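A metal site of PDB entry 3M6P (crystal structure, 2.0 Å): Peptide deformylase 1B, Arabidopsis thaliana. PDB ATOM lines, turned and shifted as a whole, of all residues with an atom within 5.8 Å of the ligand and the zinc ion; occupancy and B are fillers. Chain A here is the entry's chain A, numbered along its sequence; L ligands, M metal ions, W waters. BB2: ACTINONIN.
O4 of the ligand lies close to N of Leu 92.
The side-chain carboxylate (OE2) of Glu 134 is in hydrogen-bond range of a nitrogen (N1) of the ligand, 2.5 Å away.
The backbone NH (N) of Gly 90 lies within hydrogen-bond range of an oxygen (O20) of the ligand (3.0 Å).
The backbone NH (N) of Ile 42 is in hydrogen-bond range of an oxygen (O13) of the ligand (2.8 Å).
OE1 of Gln 48 lies within hydrogen-bond range of N1 of the ligand (3.3 Å).
A nitrogen (N14) of the ligand sits at hydrogen-bond distance from the backbone carbonyl oxygen (O) of Gly 90, at 3.2 Å.
N1 of the ligand sits close to O of Gly 43 (3.4 Å).
O of Asp 88 lies within hydrogen-bond range of O27 of the ligand, at 2.6 Å.
SG of Cys 91 sits close to NE2 of Gln 48 (3.7 Å).
OE1 of Glu 134 sits close to OE1 of Gln 48 (3.5 Å).
OG of Ser 93 sits at hydrogen-bond distance from NE2 of Gln 48 (3.2 Å).
The side-chain carboxylate (OE1) of Glu 89 lies within salt-bridge range of the guanidinium group (NE) of Arg 129.
OE2 of Glu 89 lies within hydrogen-bond range of ND1 of His 133 (2.7 Å).
The side-chain sulfur (SG) of Cys 91 lies close to the backbone NH (N) of Ser 93.
NE2 of His 137 lies close to NE2 of Gln 48, at 3.3 Å.
The side-chain amide oxygen (OE1) of Gln 48 sits at hydrogen-bond distance from the backbone NH (N) of Ser 45 (3.0 Å).
Asp 40 touches the ligand (O to C18, 3.8 Å).
CA of Gly 41 touches O13 of the ligand, at 3.2 Å.
Phe 87 touches the ligand (CE2 to O27, 3.7 Å).
C of Glu 89 touches O20 of the ligand, 3.9 Å away.
CE2 of Tyr 98 touches C17 of the ligand, at 3.3 Å.
Ile 130 touches the ligand (CA to C9, 3.7 Å).
Hydrophobic or aromatic side chains within 4 Å of the ligand: Ile 42, Phe 87, Leu 92, Tyr 98, Ile 130, His 133 and His 137.
16 residues have an atom within 4 Å of the ligand: Asp 40, Gly 41, Ile 42, Gly 43, Gln 48, Phe 87, Asp 88, Glu 89, Gly 90, Cys 91, Leu 92, Tyr 98, Ile 130, His 133, Glu 134 and His 137.
The nearest printed residue that does not touch the ligand is Leu 44 (4.1 Å).
Gln 48 touches the zinc ion (NE2 to ZN, 3.1 Å).
Four residues have an atom within 4 Å of the zinc ion: Gln 48, Cys 91, His 133 and His 137.
The nearest printed residue that does not touch the zinc ion is Leu 92 (4.3 Å).
O4 of the ligand is bound to the zinc ion, at 2.1 Å.
The side-chain sulfur (SG) of Cys 91 binds the zinc ion (2.2 Å).
The zinc ion is bound by NE2 of His 137 (2.2 Å).
NE2 of His 133 binds the zinc ion, 2.3 Å away.
The zinc ion is bound by O2 of the ligand (2.4 Å).
The zinc ion has five donor atoms within binding distance.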
ATOM      1  N   THR A  39      23.445 -35.382 -20.024  1.00  0.00           N
ATOM      2  CA  THR A  39      23.843 -34.349 -20.997  1.00  0.00           C
ATOM      3  C   THR A  39      25.080 -33.583 -20.548  1.00  0.00           C
ATOM      4  O   THR A  39      25.447 -32.585 -21.151  1.00  0.00           O
ATOM      5  CB  THR A  39      22.697 -33.340 -21.244  1.00  0.00           C
ATOM      6  OG1 THR A  39      22.327 -32.729 -19.977  1.00  0.00           O
ATOM      7  CG2 THR A  39      21.513 -34.074 -21.866  1.00  0.00           C
ATOM      8  N   ASP A  40      25.715 -34.049 -19.462  1.00  0.00           N
ATOM      9  CA  ASP A  40      26.836 -33.334 -18.822  1.00  0.00           C
ATOM     10  C   ASP A  40      26.573 -31.873 -18.399  1.00  0.00           C
ATOM     11  O   ASP A  40      27.477 -31.012 -18.481  1.00  0.00           O
ATOM     12  CB  ASP A  40      28.084 -33.405 -19.732  1.00  0.00           C
ATOM     13  CG  ASP A  40      28.368 -34.788 -20.168  1.00  0.00           C
ATOM     14  OD1 ASP A  40      28.343 -35.687 -19.295  1.00  0.00           O
ATOM     15  OD2 ASP A  40      28.588 -34.997 -21.393  1.00  0.00           O
ATOM     16  N   GLY A  41      25.383 -31.619 -17.846  1.00  0.00           N
ATOM     17  CA  GLY A  41      25.033 -30.315 -17.315  1.00  0.00           C
ATOM     18  C   GLY A  41      25.408 -30.165 -15.869  1.00  0.00           C
ATOM     19  O   GLY A  41      25.804 -31.126 -15.249  1.00  0.00           O
ATOM     20  N   ILE A  42      25.301 -28.947 -15.329  1.00  0.00           N
ATOM     21  CA  ILE A  42      25.555 -28.704 -13.933  1.00  0.00           C
ATOM     22  C   ILE A  42      24.305 -28.116 -13.271  1.00  0.00           C
ATOM     23  O   ILE A  42      24.323 -27.776 -12.121  1.00  0.00           O
ATOM     24  CB  ILE A  42      26.789 -27.840 -13.719  1.00  0.00           C
ATOM     25  CG1 ILE A  42      26.556 -26.444 -14.359  1.00  0.00           C
ATOM     26  CG2 ILE A  42      28.076 -28.636 -14.250  1.00  0.00           C
ATOM     27  CD1 ILE A  42      27.765 -25.505 -14.437  1.00  0.00           C
ATOM     28  N   GLY A  43      23.238 -27.987 -14.046  1.00  0.00           N
ATOM     29  CA  GLY A  43      21.909 -27.664 -13.565  1.00  0.00           C
ATOM     30  C   GLY A  43      20.857 -27.868 -14.634  1.00  0.00           C
ATOM     31  O   GLY A  43      21.187 -28.120 -15.819  1.00  0.00           O
ATOM     32  N   LEU A  44      19.597 -27.793 -14.199  1.00  0.00           N
ATOM     33  CA  LEU A  44      18.440 -27.862 -15.079  1.00  0.00           C
ATOM     34  C   LEU A  44      17.273 -27.159 -14.473  1.00  0.00           C
ATOM     35  O   LEU A  44      17.062 -27.175 -13.254  1.00  0.00           O
ATOM     36  CB  LEU A  44      18.034 -29.346 -15.435  1.00  0.00           C
ATOM     37  CG  LEU A  44      17.197 -29.622 -16.712  1.00  0.00           C
ATOM     38  CD1 LEU A  44      17.836 -29.153 -18.068  1.00  0.00           C
ATOM     39  CD2 LEU A  44      16.893 -31.142 -16.840  1.00  0.00           C
ATOM     40  N   SER A  45      16.439 -26.563 -15.330  1.00  0.00           N
ATOM     41  CA  SER A  45      15.178 -26.013 -14.836  1.00  0.00           C
ATOM     42  C   SER A  45      14.006 -26.691 -15.530  1.00  0.00           C
ATOM     43  O   SER A  45      14.119 -27.134 -16.682  1.00  0.00           O
ATOM     44  CB  SER A  45      15.165 -24.533 -15.099  1.00  0.00           C
ATOM     45  OG  SER A  45      15.071 -24.313 -16.498  1.00  0.00           O
ATOM     46  N   GLN A  48      12.837 -26.445 -19.226  1.00  0.00           N
ATOM     47  CA  GLN A  48      13.745 -27.154 -20.144  1.00  0.00           C
ATOM     48  C   GLN A  48      13.376 -28.608 -20.432  1.00  0.00           C
ATOM     49  O   GLN A  48      13.922 -29.186 -21.353  1.00  0.00           O
ATOM     50  CB  GLN A  48      15.171 -27.078 -19.663  1.00  0.00           C
ATOM     51  CG  GLN A  48      15.685 -25.632 -19.644  1.00  0.00           C
ATOM     52  CD  GLN A  48      17.132 -25.547 -19.190  1.00  0.00           C
ATOM     53  OE1 GLN A  48      17.427 -25.632 -18.006  1.00  0.00           O
ATOM     54  NE2 GLN A  48      18.038 -25.379 -20.149  1.00  0.00           N
ATOM     55  N   PHE A  87      31.792 -15.090 -16.882  1.00  0.00           N
ATOM     56  CA  PHE A  87      31.941 -16.561 -16.877  1.00  0.00           C
ATOM     57  C   PHE A  87      31.357 -17.008 -18.195  1.00  0.00           C
ATOM     58  O   PHE A  87      30.349 -16.450 -18.645  1.00  0.00           O
ATOM     59  CB  PHE A  87      31.220 -17.220 -15.704  1.00  0.00           C
ATOM     60  CG  PHE A  87      31.591 -18.715 -15.455  1.00  0.00           C
ATOM     61  CD1 PHE A  87      32.856 -19.078 -14.986  1.00  0.00           C
ATOM     62  CD2 PHE A  87      30.656 -19.729 -15.671  1.00  0.00           C
ATOM     63  CE1 PHE A  87      33.183 -20.421 -14.734  1.00  0.00           C
ATOM     64  CE2 PHE A  87      30.978 -21.089 -15.432  1.00  0.00           C
ATOM     65  CZ  PHE A  87      32.220 -21.431 -14.968  1.00  0.00           C
ATOM     66  N   ASP A  88      32.017 -17.958 -18.844  1.00  0.00           N
ATOM     67  CA  ASP A  88      31.522 -18.542 -20.086  1.00  0.00           C
ATOM     68  C   ASP A  88      30.442 -19.566 -19.793  1.00  0.00           C
ATOM     69  O   ASP A  88      30.705 -20.604 -19.195  1.00  0.00           O
ATOM     70  CB  ASP A  88      32.652 -19.174 -20.875  1.00  0.00           C
ATOM     71  CG  ASP A  88      33.591 -18.154 -21.398  1.00  0.00           C
ATOM     72  OD1 ASP A  88      34.402 -18.480 -22.292  1.00  0.00           O
ATOM     73  OD2 ASP A  88      33.520 -16.994 -20.923  1.00  0.00           O
ATOM     74  N   GLU A  89      29.230 -19.238 -20.232  1.00  0.00           N
ATOM     75  CA  GLU A  89      28.068 -20.110 -20.060  1.00  0.00           C
ATOM     76  C   GLU A  89      27.709 -20.755 -21.355  1.00  0.00           C
ATOM     77  O   GLU A  89      27.863 -20.151 -22.417  1.00  0.00           O
ATOM     78  CB  GLU A  89      26.853 -19.293 -19.631  1.00  0.00           C
ATOM     79  CG  GLU A  89      27.151 -18.241 -18.613  1.00  0.00           C
ATOM     80  CD  GLU A  89      25.969 -17.902 -17.730  1.00  0.00           C
ATOM     81  OE1 GLU A  89      26.206 -17.216 -16.715  1.00  0.00           O
ATOM     82  OE2 GLU A  89      24.812 -18.297 -18.056  1.00  0.00           O
ATOM     83  N   GLY A  90      27.204 -21.982 -21.241  1.00  0.00           N
ATOM     84  CA  GLY A  90      26.462 -22.649 -22.284  1.00  0.00           C
ATOM     85  C   GLY A  90      25.095 -22.971 -21.716  1.00  0.00           C
ATOM     86  O   GLY A  90      24.863 -22.924 -20.505  1.00  0.00           O
ATOM     87  N   CYS A  91      24.222 -23.476 -22.542  1.00  0.00           N
ATOM     88  CA  CYS A  91      22.915 -23.802 -22.038  1.00  0.00           C
ATOM     89  C   CYS A  91      22.444 -24.993 -22.800  1.00  0.00           C
ATOM     90  O   CYS A  91      22.607 -25.063 -24.014  1.00  0.00           O
ATOM     91  CB  CYS A  91      21.966 -22.582 -22.235  1.00  0.00           C
ATOM     92  SG  CYS A  91      20.255 -22.754 -21.633  1.00  0.00           S
ATOM     93  N   LEU A  92      21.854 -25.947 -22.081  1.00  0.00           N
ATOM     94  CA  LEU A  92      21.297 -27.180 -22.692  1.00  0.00           C
ATOM     95  C   LEU A  92      20.194 -26.897 -23.717  1.00  0.00           C
ATOM     96  O   LEU A  92      19.912 -27.729 -24.614  1.00  0.00           O
ATOM     97  CB  LEU A  92      20.778 -28.118 -21.602  1.00  0.00           C
ATOM     98  CG  LEU A  92      21.922 -28.905 -20.912  1.00  0.00           C
ATOM     99  CD1 LEU A  92      21.332 -29.814 -19.897  1.00  0.00           C
ATOM    100  CD2 LEU A  92      22.767 -29.684 -21.874  1.00  0.00           C
ATOM    101  N   SER A  93      19.567 -25.733 -23.603  1.00  0.00           N
ATOM    102  CA  SER A  93      18.546 -25.350 -24.578  1.00  0.00           C
ATOM    103  C   SER A  93      19.113 -24.705 -25.805  1.00  0.00           C
ATOM    104  O   SER A  93      18.373 -24.267 -26.667  1.00  0.00           O
ATOM    105  CB  SER A  93      17.526 -24.406 -23.985  1.00  0.00           C
ATOM    106  OG  SER A  93      16.692 -25.129 -23.071  1.00  0.00           O
ATOM    107  N   ILE A  97      26.325 -23.803 -28.040  1.00  0.00           N
ATOM    108  CA  ILE A  97      26.545 -22.342 -28.002  1.00  0.00           C
ATOM    109  C   ILE A  97      27.112 -21.944 -26.665  1.00  0.00           C
ATOM    110  O   ILE A  97      26.491 -22.264 -25.660  1.00  0.00           O
ATOM    111  CB  ILE A  97      25.238 -21.539 -28.333  1.00  0.00           C
ATOM    112  CG1 ILE A  97      24.694 -21.933 -29.730  1.00  0.00           C
ATOM    113  CG2 ILE A  97      25.485 -19.962 -28.176  1.00  0.00           C
ATOM    114  CD1 ILE A  97      23.405 -21.245 -30.068  1.00  0.00           C
ATOM    115  N   TYR A  98      28.284 -21.302 -26.635  1.00  0.00           N
ATOM    116  CA  TYR A  98      28.980 -20.883 -25.408  1.00  0.00           C
ATOM    117  C   TYR A  98      29.376 -19.417 -25.535  1.00  0.00           C
ATOM    118  O   TYR A  98      29.847 -19.001 -26.584  1.00  0.00           O
ATOM    119  CB  TYR A  98      30.259 -21.727 -25.148  1.00  0.00           C
ATOM    120  CG  TYR A  98      29.977 -23.211 -24.985  1.00  0.00           C
ATOM    121  CD1 TYR A  98      29.903 -24.064 -26.089  1.00  0.00           C
ATOM    122  CD2 TYR A  98      29.753 -23.752 -23.720  1.00  0.00           C
ATOM    123  CE1 TYR A  98      29.575 -25.424 -25.953  1.00  0.00           C
ATOM    124  CE2 TYR A  98      29.452 -25.110 -23.558  1.00  0.00           C
ATOM    125  CZ  TYR A  98      29.348 -25.942 -24.679  1.00  0.00           C
ATOM    126  OH  TYR A  98      29.038 -27.296 -24.496  1.00  0.00           O
ATOM    127  N   LEU A 126      30.420 -20.849  -8.101  1.00  0.00           N
ATOM    128  CA  LEU A 126      29.675 -21.569  -9.133  1.00  0.00           C
ATOM    129  C   LEU A 126      28.225 -21.728  -8.694  1.00  0.00           C
ATOM    130  O   LEU A 126      27.302 -21.479  -9.461  1.00  0.00           O
ATOM    131  CB  LEU A 126      30.350 -22.908  -9.475  1.00  0.00           C
ATOM    132  CG  LEU A 126      30.020 -23.607 -10.816  1.00  0.00           C
ATOM    133  CD1 LEU A 126      30.229 -22.732 -12.027  1.00  0.00           C
ATOM    134  CD2 LEU A 126      30.847 -24.842 -10.969  1.00  0.00           C
ATOM    135  N   ARG A 129      26.409 -18.691  -9.721  1.00  0.00           N
ATOM    136  CA  ARG A 129      26.387 -18.594 -11.186  1.00  0.00           C
ATOM    137  C   ARG A 129      25.306 -19.561 -11.823  1.00  0.00           C
ATOM    138  O   ARG A 129      24.513 -19.169 -12.671  1.00  0.00           O
ATOM    139  CB  ARG A 129      27.762 -18.935 -11.698  1.00  0.00           C
ATOM    140  CG  ARG A 129      27.899 -18.660 -13.157  1.00  0.00           C
ATOM    141  CD  ARG A 129      27.464 -17.197 -13.307  1.00  0.00           C
ATOM    142  NE  ARG A 129      27.762 -16.678 -14.587  1.00  0.00           N
ATOM    143  CZ  ARG A 129      28.399 -15.579 -14.856  1.00  0.00           C
ATOM    144  NH1 ARG A 129      28.837 -14.755 -13.912  1.00  0.00           N
ATOM    145  NH2 ARG A 129      28.575 -15.321 -16.143  1.00  0.00           N
ATOM    146  N   ILE A 130      25.288 -20.804 -11.383  1.00  0.00           N
ATOM    147  CA  ILE A 130      24.338 -21.777 -11.881  1.00  0.00           C
ATOM    148  C   ILE A 130      22.928 -21.333 -11.490  1.00  0.00           C
ATOM    149  O   ILE A 130      21.992 -21.351 -12.321  1.00  0.00           O
ATOM    150  CB  ILE A 130      24.600 -23.170 -11.265  1.00  0.00           C
ATOM    151  CG1 ILE A 130      25.984 -23.710 -11.655  1.00  0.00           C
ATOM    152  CG2 ILE A 130      23.510 -24.132 -11.665  1.00  0.00           C
ATOM    153  CD1 ILE A 130      26.385 -24.982 -10.876  1.00  0.00           C
ATOM    154  N   HIS A 133      21.669 -18.358 -13.636  1.00  0.00           N
ATOM    155  CA  HIS A 133      21.292 -19.034 -14.913  1.00  0.00           C
ATOM    156  C   HIS A 133      19.906 -19.745 -14.907  1.00  0.00           C
ATOM    157  O   HIS A 133      19.058 -19.492 -15.777  1.00  0.00           O
ATOM    158  CB  HIS A 133      22.341 -20.037 -15.343  1.00  0.00           C
ATOM    159  CG  HIS A 133      22.116 -20.573 -16.721  1.00  0.00           C
ATOM    160  ND1 HIS A 133      22.850 -20.141 -17.814  1.00  0.00           N
ATOM    161  CD2 HIS A 133      21.253 -21.509 -17.187  1.00  0.00           C
ATOM    162  CE1 HIS A 133      22.444 -20.813 -18.891  1.00  0.00           C
ATOM    163  NE2 HIS A 133      21.453 -21.614 -18.532  1.00  0.00           N
ATOM    164  N   GLU A 134      19.681 -20.604 -13.912  1.00  0.00           N
ATOM    165  CA  GLU A 134      18.453 -21.423 -13.818  1.00  0.00           C
ATOM    166  C   GLU A 134      17.241 -20.584 -13.320  1.00  0.00           C
ATOM    167  O   GLU A 134      16.104 -20.807 -13.710  1.00  0.00           O
ATOM    168  CB  GLU A 134      18.629 -22.577 -12.851  1.00  0.00           C
ATOM    169  CG  GLU A 134      19.755 -23.526 -13.020  1.00  0.00           C
ATOM    170  CD  GLU A 134      19.778 -24.194 -14.382  1.00  0.00           C
ATOM    171  OE1 GLU A 134      18.696 -24.383 -15.018  1.00  0.00           O
ATOM    172  OE2 GLU A 134      20.892 -24.581 -14.793  1.00  0.00           O
ATOM    173  N   HIS A 137      15.779 -18.904 -16.047  1.00  0.00           N
ATOM    174  CA  HIS A 137      14.876 -19.787 -16.758  1.00  0.00           C
ATOM    175  C   HIS A 137      13.475 -19.794 -16.125  1.00  0.00           C
ATOM    176  O   HIS A 137      12.454 -19.865 -16.822  1.00  0.00           O
ATOM    177  CB  HIS A 137      15.440 -21.197 -16.774  1.00  0.00           C
ATOM    178  CG  HIS A 137      16.377 -21.486 -17.920  1.00  0.00           C
ATOM    179  ND1 HIS A 137      15.962 -21.503 -19.229  1.00  0.00           N
ATOM    180  CD2 HIS A 137      17.653 -21.942 -17.920  1.00  0.00           C
ATOM    181  CE1 HIS A 137      16.976 -21.834 -20.014  1.00  0.00           C
ATOM    182  NE2 HIS A 137      18.001 -22.171 -19.251  1.00  0.00           N
HETATM  183  C5  BB2 L   1      22.435 -26.325 -18.068  1.00  0.00           C
HETATM  184  C3  BB2 L   1      21.293 -25.381 -18.259  1.00  0.00           C
HETATM  185  O4  BB2 L   1      21.121 -24.914 -19.359  1.00  0.00           O
HETATM  186  N1  BB2 L   1      20.556 -25.075 -17.187  1.00  0.00           N
HETATM  187  O2  BB2 L   1      19.535 -24.188 -17.401  1.00  0.00           O
HETATM  188  C6  BB2 L   1      23.634 -25.365 -18.126  1.00  0.00           C
HETATM  189  C12 BB2 L   1      24.910 -26.138 -18.204  1.00  0.00           C
HETATM  190  O13 BB2 L   1      25.086 -27.135 -17.497  1.00  0.00           O
HETATM  191  C7  BB2 L   1      23.723 -24.546 -16.756  1.00  0.00           C
HETATM  192  C8  BB2 L   1      25.002 -23.651 -16.679  1.00  0.00           C
HETATM  193  C9  BB2 L   1      25.059 -22.910 -15.370  1.00  0.00           C
HETATM  194  C10 BB2 L   1      26.033 -21.662 -15.534  1.00  0.00           C
HETATM  195  C11 BB2 L   1      27.422 -22.034 -16.132  1.00  0.00           C
HETATM  196  N14 BB2 L   1      25.771 -25.647 -19.045  1.00  0.00           N
HETATM  197  C15 BB2 L   1      27.087 -26.240 -19.166  1.00  0.00           C
HETATM  198  C16 BB2 L   1      27.321 -26.881 -20.536  1.00  0.00           C
HETATM  199  C18 BB2 L   1      26.371 -28.112 -20.682  1.00  0.00           C
HETATM  200  C17 BB2 L   1      26.969 -25.910 -21.604  1.00  0.00           C
HETATM  201  C19 BB2 L   1      28.121 -25.127 -18.812  1.00  0.00           C
HETATM  202  O20 BB2 L   1      27.889 -23.937 -19.086  1.00  0.00           O
HETATM  203  N21 BB2 L   1      29.278 -25.465 -18.167  1.00  0.00           N
HETATM  204  C22 BB2 L   1      30.312 -24.503 -17.785  1.00  0.00           C
HETATM  205  C23 BB2 L   1      29.659 -26.835 -17.759  1.00  0.00           C
HETATM  206  C24 BB2 L   1      30.634 -26.611 -16.602  1.00  0.00           C
HETATM  207  C25 BB2 L   1      31.291 -25.277 -16.904  1.00  0.00           C
HETATM  208  C26 BB2 L   1      31.092 -23.987 -19.025  1.00  0.00           C
HETATM  209  O27 BB2 L   1      31.843 -22.853 -18.570  1.00  0.00           O
HETATM  210 ZN    ZN M   1      20.017 -23.115 -19.452  1.00  0.00          ZN
HETATM  211  O   HOH W   1      34.493 -22.901 -17.349  1.00  0.00           O
HETATM  212  O   HOH W   2      32.425 -29.441 -17.307  1.00  0.00           O
